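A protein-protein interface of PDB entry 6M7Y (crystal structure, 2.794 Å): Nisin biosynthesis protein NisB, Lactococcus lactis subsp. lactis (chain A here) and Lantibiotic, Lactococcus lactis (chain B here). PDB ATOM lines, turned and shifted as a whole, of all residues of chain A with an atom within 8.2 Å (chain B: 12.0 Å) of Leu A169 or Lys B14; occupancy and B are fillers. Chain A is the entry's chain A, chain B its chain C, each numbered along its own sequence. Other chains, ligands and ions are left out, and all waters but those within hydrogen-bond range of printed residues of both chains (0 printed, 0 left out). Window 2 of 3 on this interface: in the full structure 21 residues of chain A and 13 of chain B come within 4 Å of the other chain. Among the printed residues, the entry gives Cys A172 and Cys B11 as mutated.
O of Glu A171 lies within hydrogen-bond range of N of Val B12 (3.0 Å).
The side-chain sulfur (SG) of Cys A172 is disulfide-bonded to the side-chain sulfur (SG) of Cys B11 (2.1 Å).
OE1 of Glu A505 is in salt-bridge range of NZ of Lys B14 (3.6 Å).
O of Leu A169 sits close to O of Ser B13 (3.4 Å).
The side-chain hydroxyl of Thr A163 is in hydrogen-bond range of the backbone NH of Cys A172 (3.3 Å).
The side-chain hydroxyl (OG) of Ser A166 sits at hydrogen-bond distance from the side-chain carboxylate (OE2) of Glu A170 (3.3 Å).
The side-chain carboxylate (OE1) of Glu A168 lies within hydrogen-bond range of the backbone NH (N) of Glu A170 (2.6 Å).
Lys B14 touches Leu A169.
Glu A170 touches Cys B11.
CB of Glu A170 touches O of Val B12, at 3.1 Å.
Glu A170 touches Ser B13.
Glu A170 touches Lys B14.
O of Glu A171 touches CA of Cys B11, 3.2 Å away.
Val B10 touches Cys A172.
Leu A169 touches two residues of chain B.
No residue of chain B comes within 4 Å of Thr A163.
No residue of chain B comes within 4 Å of Ser A166.
No residue of chain B comes within 4 Å of Glu A168.
Of the printed residues of chain B, Glu A170 touches Cys B11, Val B12, Ser B13 and Lys B14.
Printed residues of chain B within 4 Å of Glu A171: Cys B11 (3.2 Å) and Val B12 (3.0 Å).
Ser B13 touches just these residues of chain A: Leu A169 (3.4 Å) and Glu A170 (3.4 Å).
Of the printed residues of chain B, Cys A172 touches Val B10 and Cys B11.
Of the printed residues of chain A, Val B12 touches Glu A170 and Glu A171.
Of the printed residues of chain B, Glu A505 touches Lys B14.
Printed residues of chain A within 4 Å of Cys B11: Glu A170, Glu A171 and Cys A172.
Ile A507 touches none of the printed residues of chain B.
The nearest residue of chain B that does not touch Leu A169 is Val B12 (5.2 Å).
Of the 5 printed residues of chain B, 5 touch a printed residue of chain A.
Among the printed residues, 11 pairs touch across the chains.
Among the printed residues, Asp or Glu carboxylates within 4 Å of a Lys or Arg side-chain nitrogen of the other chain: Glu A505 with Lys B14 (3.6 Å).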
ATOM      1  N   TYR A 162      -1.306 -11.394  -5.939  1.00  0.00           N
ATOM      2  CA  TYR A 162      -2.255 -10.489  -6.572  1.00  0.00           C
ATOM      3  C   TYR A 162      -2.547  -9.369  -5.589  1.00  0.00           C
ATOM      4  O   TYR A 162      -2.118  -9.419  -4.439  1.00  0.00           O
ATOM      5  CB  TYR A 162      -3.514 -11.226  -7.036  1.00  0.00           C
ATOM      6  CG  TYR A 162      -4.248 -11.990  -5.971  1.00  0.00           C
ATOM      7  CD1 TYR A 162      -3.938 -13.313  -5.722  1.00  0.00           C
ATOM      8  CD2 TYR A 162      -5.277 -11.394  -5.226  1.00  0.00           C
ATOM      9  CE1 TYR A 162      -4.615 -14.030  -4.764  1.00  0.00           C
ATOM     10  CE2 TYR A 162      -5.966 -12.097  -4.267  1.00  0.00           C
ATOM     11  CZ  TYR A 162      -5.626 -13.422  -4.037  1.00  0.00           C
ATOM     12  OH  TYR A 162      -6.282 -14.163  -3.093  1.00  0.00           O
ATOM     13  N   THR A 163      -3.281  -8.354  -6.052  1.00  0.00           N
ATOM     14  CA  THR A 163      -3.397  -7.065  -5.367  1.00  0.00           C
ATOM     15  C   THR A 163      -4.868  -6.741  -5.111  1.00  0.00           C
ATOM     16  O   THR A 163      -5.755  -7.353  -5.711  1.00  0.00           O
ATOM     17  CB  THR A 163      -2.697  -5.978  -6.214  1.00  0.00           C
ATOM     18  OG1 THR A 163      -1.281  -6.228  -6.217  1.00  0.00           O
ATOM     19  CG2 THR A 163      -2.947  -4.556  -5.703  1.00  0.00           C
ATOM     20  N   ILE A 164      -5.146  -5.802  -4.184  1.00  0.00           N
ATOM     21  CA  ILE A 164      -6.540  -5.441  -3.896  1.00  0.00           C
ATOM     22  C   ILE A 164      -6.833  -3.938  -3.733  1.00  0.00           C
ATOM     23  O   ILE A 164      -7.571  -3.378  -4.559  1.00  0.00           O
ATOM     24  CB  ILE A 164      -7.051  -6.238  -2.678  1.00  0.00           C
ATOM     25  CG1 ILE A 164      -7.106  -7.729  -3.038  1.00  0.00           C
ATOM     26  CG2 ILE A 164      -8.421  -5.754  -2.248  1.00  0.00           C
ATOM     27  CD1 ILE A 164      -8.115  -8.512  -2.300  1.00  0.00           C
ATOM     28  N   SER A 166      -6.330  -0.659  -4.055  1.00  0.00           N
ATOM     29  CA  SER A 166      -6.669   0.237  -5.152  1.00  0.00           C
ATOM     30  C   SER A 166      -7.877  -0.350  -5.874  1.00  0.00           C
ATOM     31  O   SER A 166      -7.726  -1.203  -6.757  1.00  0.00           O
ATOM     32  CB  SER A 166      -5.482   0.424  -6.101  1.00  0.00           C
ATOM     33  OG  SER A 166      -5.871   1.113  -7.277  1.00  0.00           O
ATOM     34  N   SER A 167      -9.080   0.061  -5.449  1.00  0.00           N
ATOM     35  CA  SER A 167     -10.330  -0.483  -5.974  1.00  0.00           C
ATOM     36  C   SER A 167     -10.406  -0.221  -7.472  1.00  0.00           C
ATOM     37  O   SER A 167     -10.971   0.781  -7.920  1.00  0.00           O
ATOM     38  CB  SER A 167     -11.537   0.114  -5.246  1.00  0.00           C
ATOM     39  OG  SER A 167     -11.526  -0.228  -3.872  1.00  0.00           O
ATOM     40  N   GLU A 168      -9.848  -1.146  -8.241  1.00  0.00           N
ATOM     41  CA  GLU A 168      -9.447  -0.887  -9.608  1.00  0.00           C
ATOM     42  C   GLU A 168      -9.021  -2.249 -10.167  1.00  0.00           C
ATOM     43  O   GLU A 168      -9.435  -3.285  -9.650  1.00  0.00           O
ATOM     44  CB  GLU A 168      -8.403   0.254  -9.598  1.00  0.00           C
ATOM     45  CG  GLU A 168      -7.867   0.800 -10.929  1.00  0.00           C
ATOM     46  CD  GLU A 168      -6.731  -0.040 -11.418  1.00  0.00           C
ATOM     47  OE1 GLU A 168      -6.298  -0.842 -10.568  1.00  0.00           O
ATOM     48  OE2 GLU A 168      -6.322   0.031 -12.602  1.00  0.00           O
ATOM     49  N   LEU A 169      -8.223  -2.244 -11.249  1.00  0.00           N
ATOM     50  CA  LEU A 169      -7.522  -3.437 -11.746  1.00  0.00           C
ATOM     51  C   LEU A 169      -6.085  -3.016 -12.161  1.00  0.00           C
ATOM     52  O   LEU A 169      -5.806  -2.618 -13.300  1.00  0.00           O
ATOM     53  CB  LEU A 169      -8.315  -4.110 -12.866  1.00  0.00           C
ATOM     54  CG  LEU A 169      -9.535  -4.957 -12.435  1.00  0.00           C
ATOM     55  CD1 LEU A 169     -10.756  -4.790 -13.373  1.00  0.00           C
ATOM     56  CD2 LEU A 169      -9.182  -6.450 -12.260  1.00  0.00           C
ATOM     57  N   GLU A 170      -5.166  -3.048 -11.181  1.00  0.00           N
ATOM     58  CA  GLU A 170      -3.745  -2.745 -11.364  1.00  0.00           C
ATOM     59  C   GLU A 170      -2.965  -3.331 -10.187  1.00  0.00           C
ATOM     60  O   GLU A 170      -3.424  -3.281  -9.039  1.00  0.00           O
ATOM     61  CB  GLU A 170      -3.465  -1.230 -11.486  1.00  0.00           C
ATOM     62  CG  GLU A 170      -3.277  -0.456 -10.165  1.00  0.00           C
ATOM     63  CD  GLU A 170      -3.083   1.050 -10.373  1.00  0.00           C
ATOM     64  OE1 GLU A 170      -2.400   1.445 -11.345  1.00  0.00           O
ATOM     65  OE2 GLU A 170      -3.633   1.839  -9.566  1.00  0.00           O
ATOM     66  N   GLU A 171      -1.787  -3.887 -10.489  1.00  0.00           N
ATOM     67  CA  GLU A 171      -0.912  -4.530  -9.515  1.00  0.00           C
ATOM     68  C   GLU A 171       0.059  -3.531  -8.878  1.00  0.00           C
ATOM     69  O   GLU A 171       0.538  -2.595  -9.523  1.00  0.00           O
ATOM     70  CB  GLU A 171      -0.136  -5.668 -10.183  1.00  0.00           C
ATOM     71  CG  GLU A 171      -0.800  -7.027 -10.077  1.00  0.00           C
ATOM     72  CD  GLU A 171       0.166  -8.159 -10.416  1.00  0.00           C
ATOM     73  OE1 GLU A 171       0.806  -8.086 -11.491  1.00  0.00           O
ATOM     74  OE2 GLU A 171       0.299  -9.108  -9.605  1.00  0.00           O
ATOM     75  N   CYS A 172       0.367  -3.753  -7.600  1.00  0.00           N
ATOM     76  CA  CYS A 172       1.169  -2.818  -6.818  1.00  0.00           C
ATOM     77  C   CYS A 172       2.188  -3.571  -5.969  1.00  0.00           C
ATOM     78  O   CYS A 172       1.851  -4.591  -5.359  1.00  0.00           O
ATOM     79  CB  CYS A 172       0.257  -1.951  -5.922  1.00  0.00           C
ATOM     80  SG  CYS A 172      -0.877  -0.807  -6.818  1.00  0.00           S
ATOM     81  N   ASN A 374      -3.218 -16.571 -18.260  1.00  0.00           N
ATOM     82  CA  ASN A 374      -3.415 -15.152 -18.555  1.00  0.00           C
ATOM     83  C   ASN A 374      -3.262 -14.220 -17.357  1.00  0.00           C
ATOM     84  O   ASN A 374      -3.678 -13.061 -17.453  1.00  0.00           O
ATOM     85  CB  ASN A 374      -4.804 -14.928 -19.162  1.00  0.00           C
ATOM     86  CG  ASN A 374      -4.998 -15.694 -20.438  1.00  0.00           C
ATOM     87  OD1 ASN A 374      -4.446 -15.338 -21.484  1.00  0.00           O
ATOM     88  ND2 ASN A 374      -5.760 -16.776 -20.362  1.00  0.00           N
ATOM     89  N   HIS A 375      -2.705 -14.678 -16.234  1.00  0.00           N
ATOM     90  CA  HIS A 375      -2.632 -13.824 -15.038  1.00  0.00           C
ATOM     91  C   HIS A 375      -1.244 -13.869 -14.369  1.00  0.00           C
ATOM     92  O   HIS A 375      -1.082 -14.468 -13.289  1.00  0.00           O
ATOM     93  CB  HIS A 375      -3.736 -14.204 -14.007  1.00  0.00           C
ATOM     94  CG  HIS A 375      -5.123 -14.221 -14.583  1.00  0.00           C
ATOM     95  ND1 HIS A 375      -5.748 -13.090 -15.064  1.00  0.00           N
ATOM     96  CD2 HIS A 375      -5.995 -15.241 -14.785  1.00  0.00           C
ATOM     97  CE1 HIS A 375      -6.941 -13.412 -15.537  1.00  0.00           C
ATOM     98  NE2 HIS A 375      -7.120 -14.709 -15.374  1.00  0.00           N
ATOM     99  N   PRO A 376      -0.245 -13.202 -14.986  1.00  0.00           N
ATOM    100  CA  PRO A 376      -0.336 -12.462 -16.258  1.00  0.00           C
ATOM    101  C   PRO A 376      -0.018 -13.342 -17.473  1.00  0.00           C
ATOM    102  O   PRO A 376       0.613 -14.395 -17.303  1.00  0.00           O
ATOM    103  CB  PRO A 376       0.724 -11.382 -16.092  1.00  0.00           C
ATOM    104  CG  PRO A 376       1.778 -12.048 -15.295  1.00  0.00           C
ATOM    105  CD  PRO A 376       1.082 -13.028 -14.362  1.00  0.00           C
ATOM    106  N   ARG A 377      -0.443 -12.942 -18.674  1.00  0.00           N
ATOM    107  CA  ARG A 377       0.064 -13.605 -19.871  1.00  0.00           C
ATOM    108  C   ARG A 377       1.571 -13.356 -19.973  1.00  0.00           C
ATOM    109  O   ARG A 377       2.087 -12.362 -19.455  1.00  0.00           O
ATOM    110  CB  ARG A 377      -0.685 -13.091 -21.111  1.00  0.00           C
ATOM    111  CG  ARG A 377      -0.379 -13.811 -22.431  1.00  0.00           C
ATOM    112  CD  ARG A 377      -0.970 -13.056 -23.654  1.00  0.00           C
ATOM    113  NE  ARG A 377      -2.296 -13.544 -24.053  1.00  0.00           N
ATOM    114  CZ  ARG A 377      -3.461 -13.103 -23.562  1.00  0.00           C
ATOM    115  NH1 ARG A 377      -3.507 -12.142 -22.636  1.00  0.00           N
ATOM    116  NH2 ARG A 377      -4.598 -13.632 -24.001  1.00  0.00           N
ATOM    117  N   GLU A 505      -9.583 -11.740  -6.275  1.00  0.00           N
ATOM    118  CA  GLU A 505      -8.917 -10.473  -6.554  1.00  0.00           C
ATOM    119  C   GLU A 505      -9.943  -9.391  -6.828  1.00  0.00           C
ATOM    120  O   GLU A 505      -9.785  -8.246  -6.385  1.00  0.00           O
ATOM    121  CB  GLU A 505      -7.935 -10.621  -7.719  1.00  0.00           C
ATOM    122  CG  GLU A 505      -7.666  -9.347  -8.497  1.00  0.00           C
ATOM    123  CD  GLU A 505      -6.481  -9.480  -9.446  1.00  0.00           C
ATOM    124  OE1 GLU A 505      -5.711  -8.496  -9.607  1.00  0.00           O
ATOM    125  OE2 GLU A 505      -6.300 -10.586 -10.001  1.00  0.00           O
ATOM    126  N   ASN A 506     -11.014  -9.747  -7.521  1.00  0.00           N
ATOM    127  CA  ASN A 506     -12.158  -8.870  -7.713  1.00  0.00           C
ATOM    128  C   ASN A 506     -13.204  -9.274  -6.675  1.00  0.00           C
ATOM    129  O   ASN A 506     -13.806 -10.349  -6.786  1.00  0.00           O
ATOM    130  CB  ASN A 506     -12.677  -8.999  -9.143  1.00  0.00           C
ATOM    131  CG  ASN A 506     -13.945  -8.213  -9.380  1.00  0.00           C
ATOM    132  OD1 ASN A 506     -14.865  -8.688 -10.043  1.00  0.00           O
ATOM    133  ND2 ASN A 506     -14.003  -6.998  -8.841  1.00  0.00           N
ATOM    134  N   ILE A 507     -13.406  -8.430  -5.651  1.00  0.00           N
ATOM    135  CA  ILE A 507     -14.136  -8.899  -4.468  1.00  0.00           C
ATOM    136  C   ILE A 507     -15.629  -9.050  -4.706  1.00  0.00           C
ATOM    137  O   ILE A 507     -16.322  -9.563  -3.820  1.00  0.00           O
ATOM    138  CB  ILE A 507     -13.934  -8.029  -3.203  1.00  0.00           C
ATOM    139  CG1 ILE A 507     -14.362  -6.573  -3.433  1.00  0.00           C
ATOM    140  CG2 ILE A 507     -12.470  -8.123  -2.684  1.00  0.00           C
ATOM    141  CD1 ILE A 507     -13.901  -5.604  -2.323  1.00  0.00           C
ATOM    142  N   ARG A 508     -16.143  -8.656  -5.880  1.00  0.00           N
ATOM    143  CA  ARG A 508     -17.526  -8.988  -6.236  1.00  0.00           C
ATOM    144  C   ARG A 508     -17.746 -10.491  -6.215  1.00  0.00           C
ATOM    145  O   ARG A 508     -18.736 -10.981  -5.665  1.00  0.00           O
ATOM    146  CB  ARG A 508     -17.867  -8.444  -7.617  1.00  0.00           C
ATOM    147  CG  ARG A 508     -17.767  -6.937  -7.723  1.00  0.00           C
ATOM    148  CD  ARG A 508     -17.171  -6.544  -9.069  1.00  0.00           C
ATOM    149  NE  ARG A 508     -16.588  -5.204  -9.052  1.00  0.00           N
ATOM    150  CZ  ARG A 508     -15.842  -4.696 -10.029  1.00  0.00           C
ATOM    151  NH1 ARG A 508     -15.569  -5.422 -11.112  1.00  0.00           N
ATOM    152  NH2 ARG A 508     -15.364  -3.461  -9.919  1.00  0.00           N
ATOM    153  N   VAL B  10       4.823   1.361  -6.073  1.00  0.00           N
ATOM    154  CA  VAL B  10       4.748   1.565  -7.515  1.00  0.00           C
ATOM    155  C   VAL B  10       3.670   0.634  -8.053  1.00  0.00           C
ATOM    156  O   VAL B  10       3.482  -0.480  -7.546  1.00  0.00           O
ATOM    157  CB  VAL B  10       6.110   1.327  -8.217  1.00  0.00           C
ATOM    158  CG1 VAL B  10       7.240   1.885  -7.381  1.00  0.00           C
ATOM    159  CG2 VAL B  10       6.349  -0.107  -8.527  1.00  0.00           C
ATOM    160  N   CYS B  11       2.927   1.111  -9.042  1.00  0.00           N
ATOM    161  CA  CYS B  11       1.809   0.369  -9.592  1.00  0.00           C
ATOM    162  C   CYS B  11       1.923   0.374 -11.105  1.00  0.00           C
ATOM    163  O   CYS B  11       2.393   1.349 -11.696  1.00  0.00           O
ATOM    164  CB  CYS B  11       0.463   0.958  -9.134  1.00  0.00           C
ATOM    165  SG  CYS B  11       0.210   0.888  -7.312  1.00  0.00           S
ATOM    166  N   VAL B  12       1.518  -0.741 -11.723  1.00  0.00           N
ATOM    167  CA  VAL B  12       1.596  -0.937 -13.166  1.00  0.00           C
ATOM    168  C   VAL B  12       0.210  -1.328 -13.672  1.00  0.00           C
ATOM    169  O   VAL B  12      -0.679  -1.656 -12.890  1.00  0.00           O
ATOM    170  CB  VAL B  12       2.651  -1.993 -13.552  1.00  0.00           C
ATOM    171  CG1 VAL B  12       4.036  -1.519 -13.139  1.00  0.00           C
ATOM    172  CG2 VAL B  12       2.328  -3.326 -12.902  1.00  0.00           C
ATOM    173  N   SER B  13       0.045  -1.310 -15.007  1.00  0.00           N
ATOM    174  CA  SER B  13      -1.274  -1.297 -15.649  1.00  0.00           C
ATOM    175  C   SER B  13      -1.992  -2.643 -15.569  1.00  0.00           C
ATOM    176  O   SER B  13      -2.667  -2.874 -14.571  1.00  0.00           O
ATOM    177  CB  SER B  13      -1.155  -0.828 -17.107  1.00  0.00           C
ATOM    178  OG  SER B  13      -2.126   0.173 -17.412  1.00  0.00           O
ATOM    179  N   LYS B  14      -1.900  -3.499 -16.603  1.00  0.00           N
ATOM    180  CA  LYS B  14      -2.497  -4.865 -16.659  1.00  0.00           C
ATOM    181  C   LYS B  14      -1.972  -5.685 -17.850  1.00  0.00           C
ATOM    182  O   LYS B  14      -2.744  -6.081 -18.749  1.00  0.00           O
ATOM    183  CB  LYS B  14      -4.029  -4.845 -16.761  1.00  0.00           C
ATOM    184  CG  LYS B  14      -4.766  -4.595 -15.496  1.00  0.00           C
ATOM    185  CD  LYS B  14      -4.152  -5.275 -14.288  1.00  0.00           C
ATOM    186  CE  LYS B  14      -4.680  -6.588 -13.966  1.00  0.00           C
ATOM    187  NZ  LYS B  14      -4.757  -6.683 -12.520  1.00  0.00           N
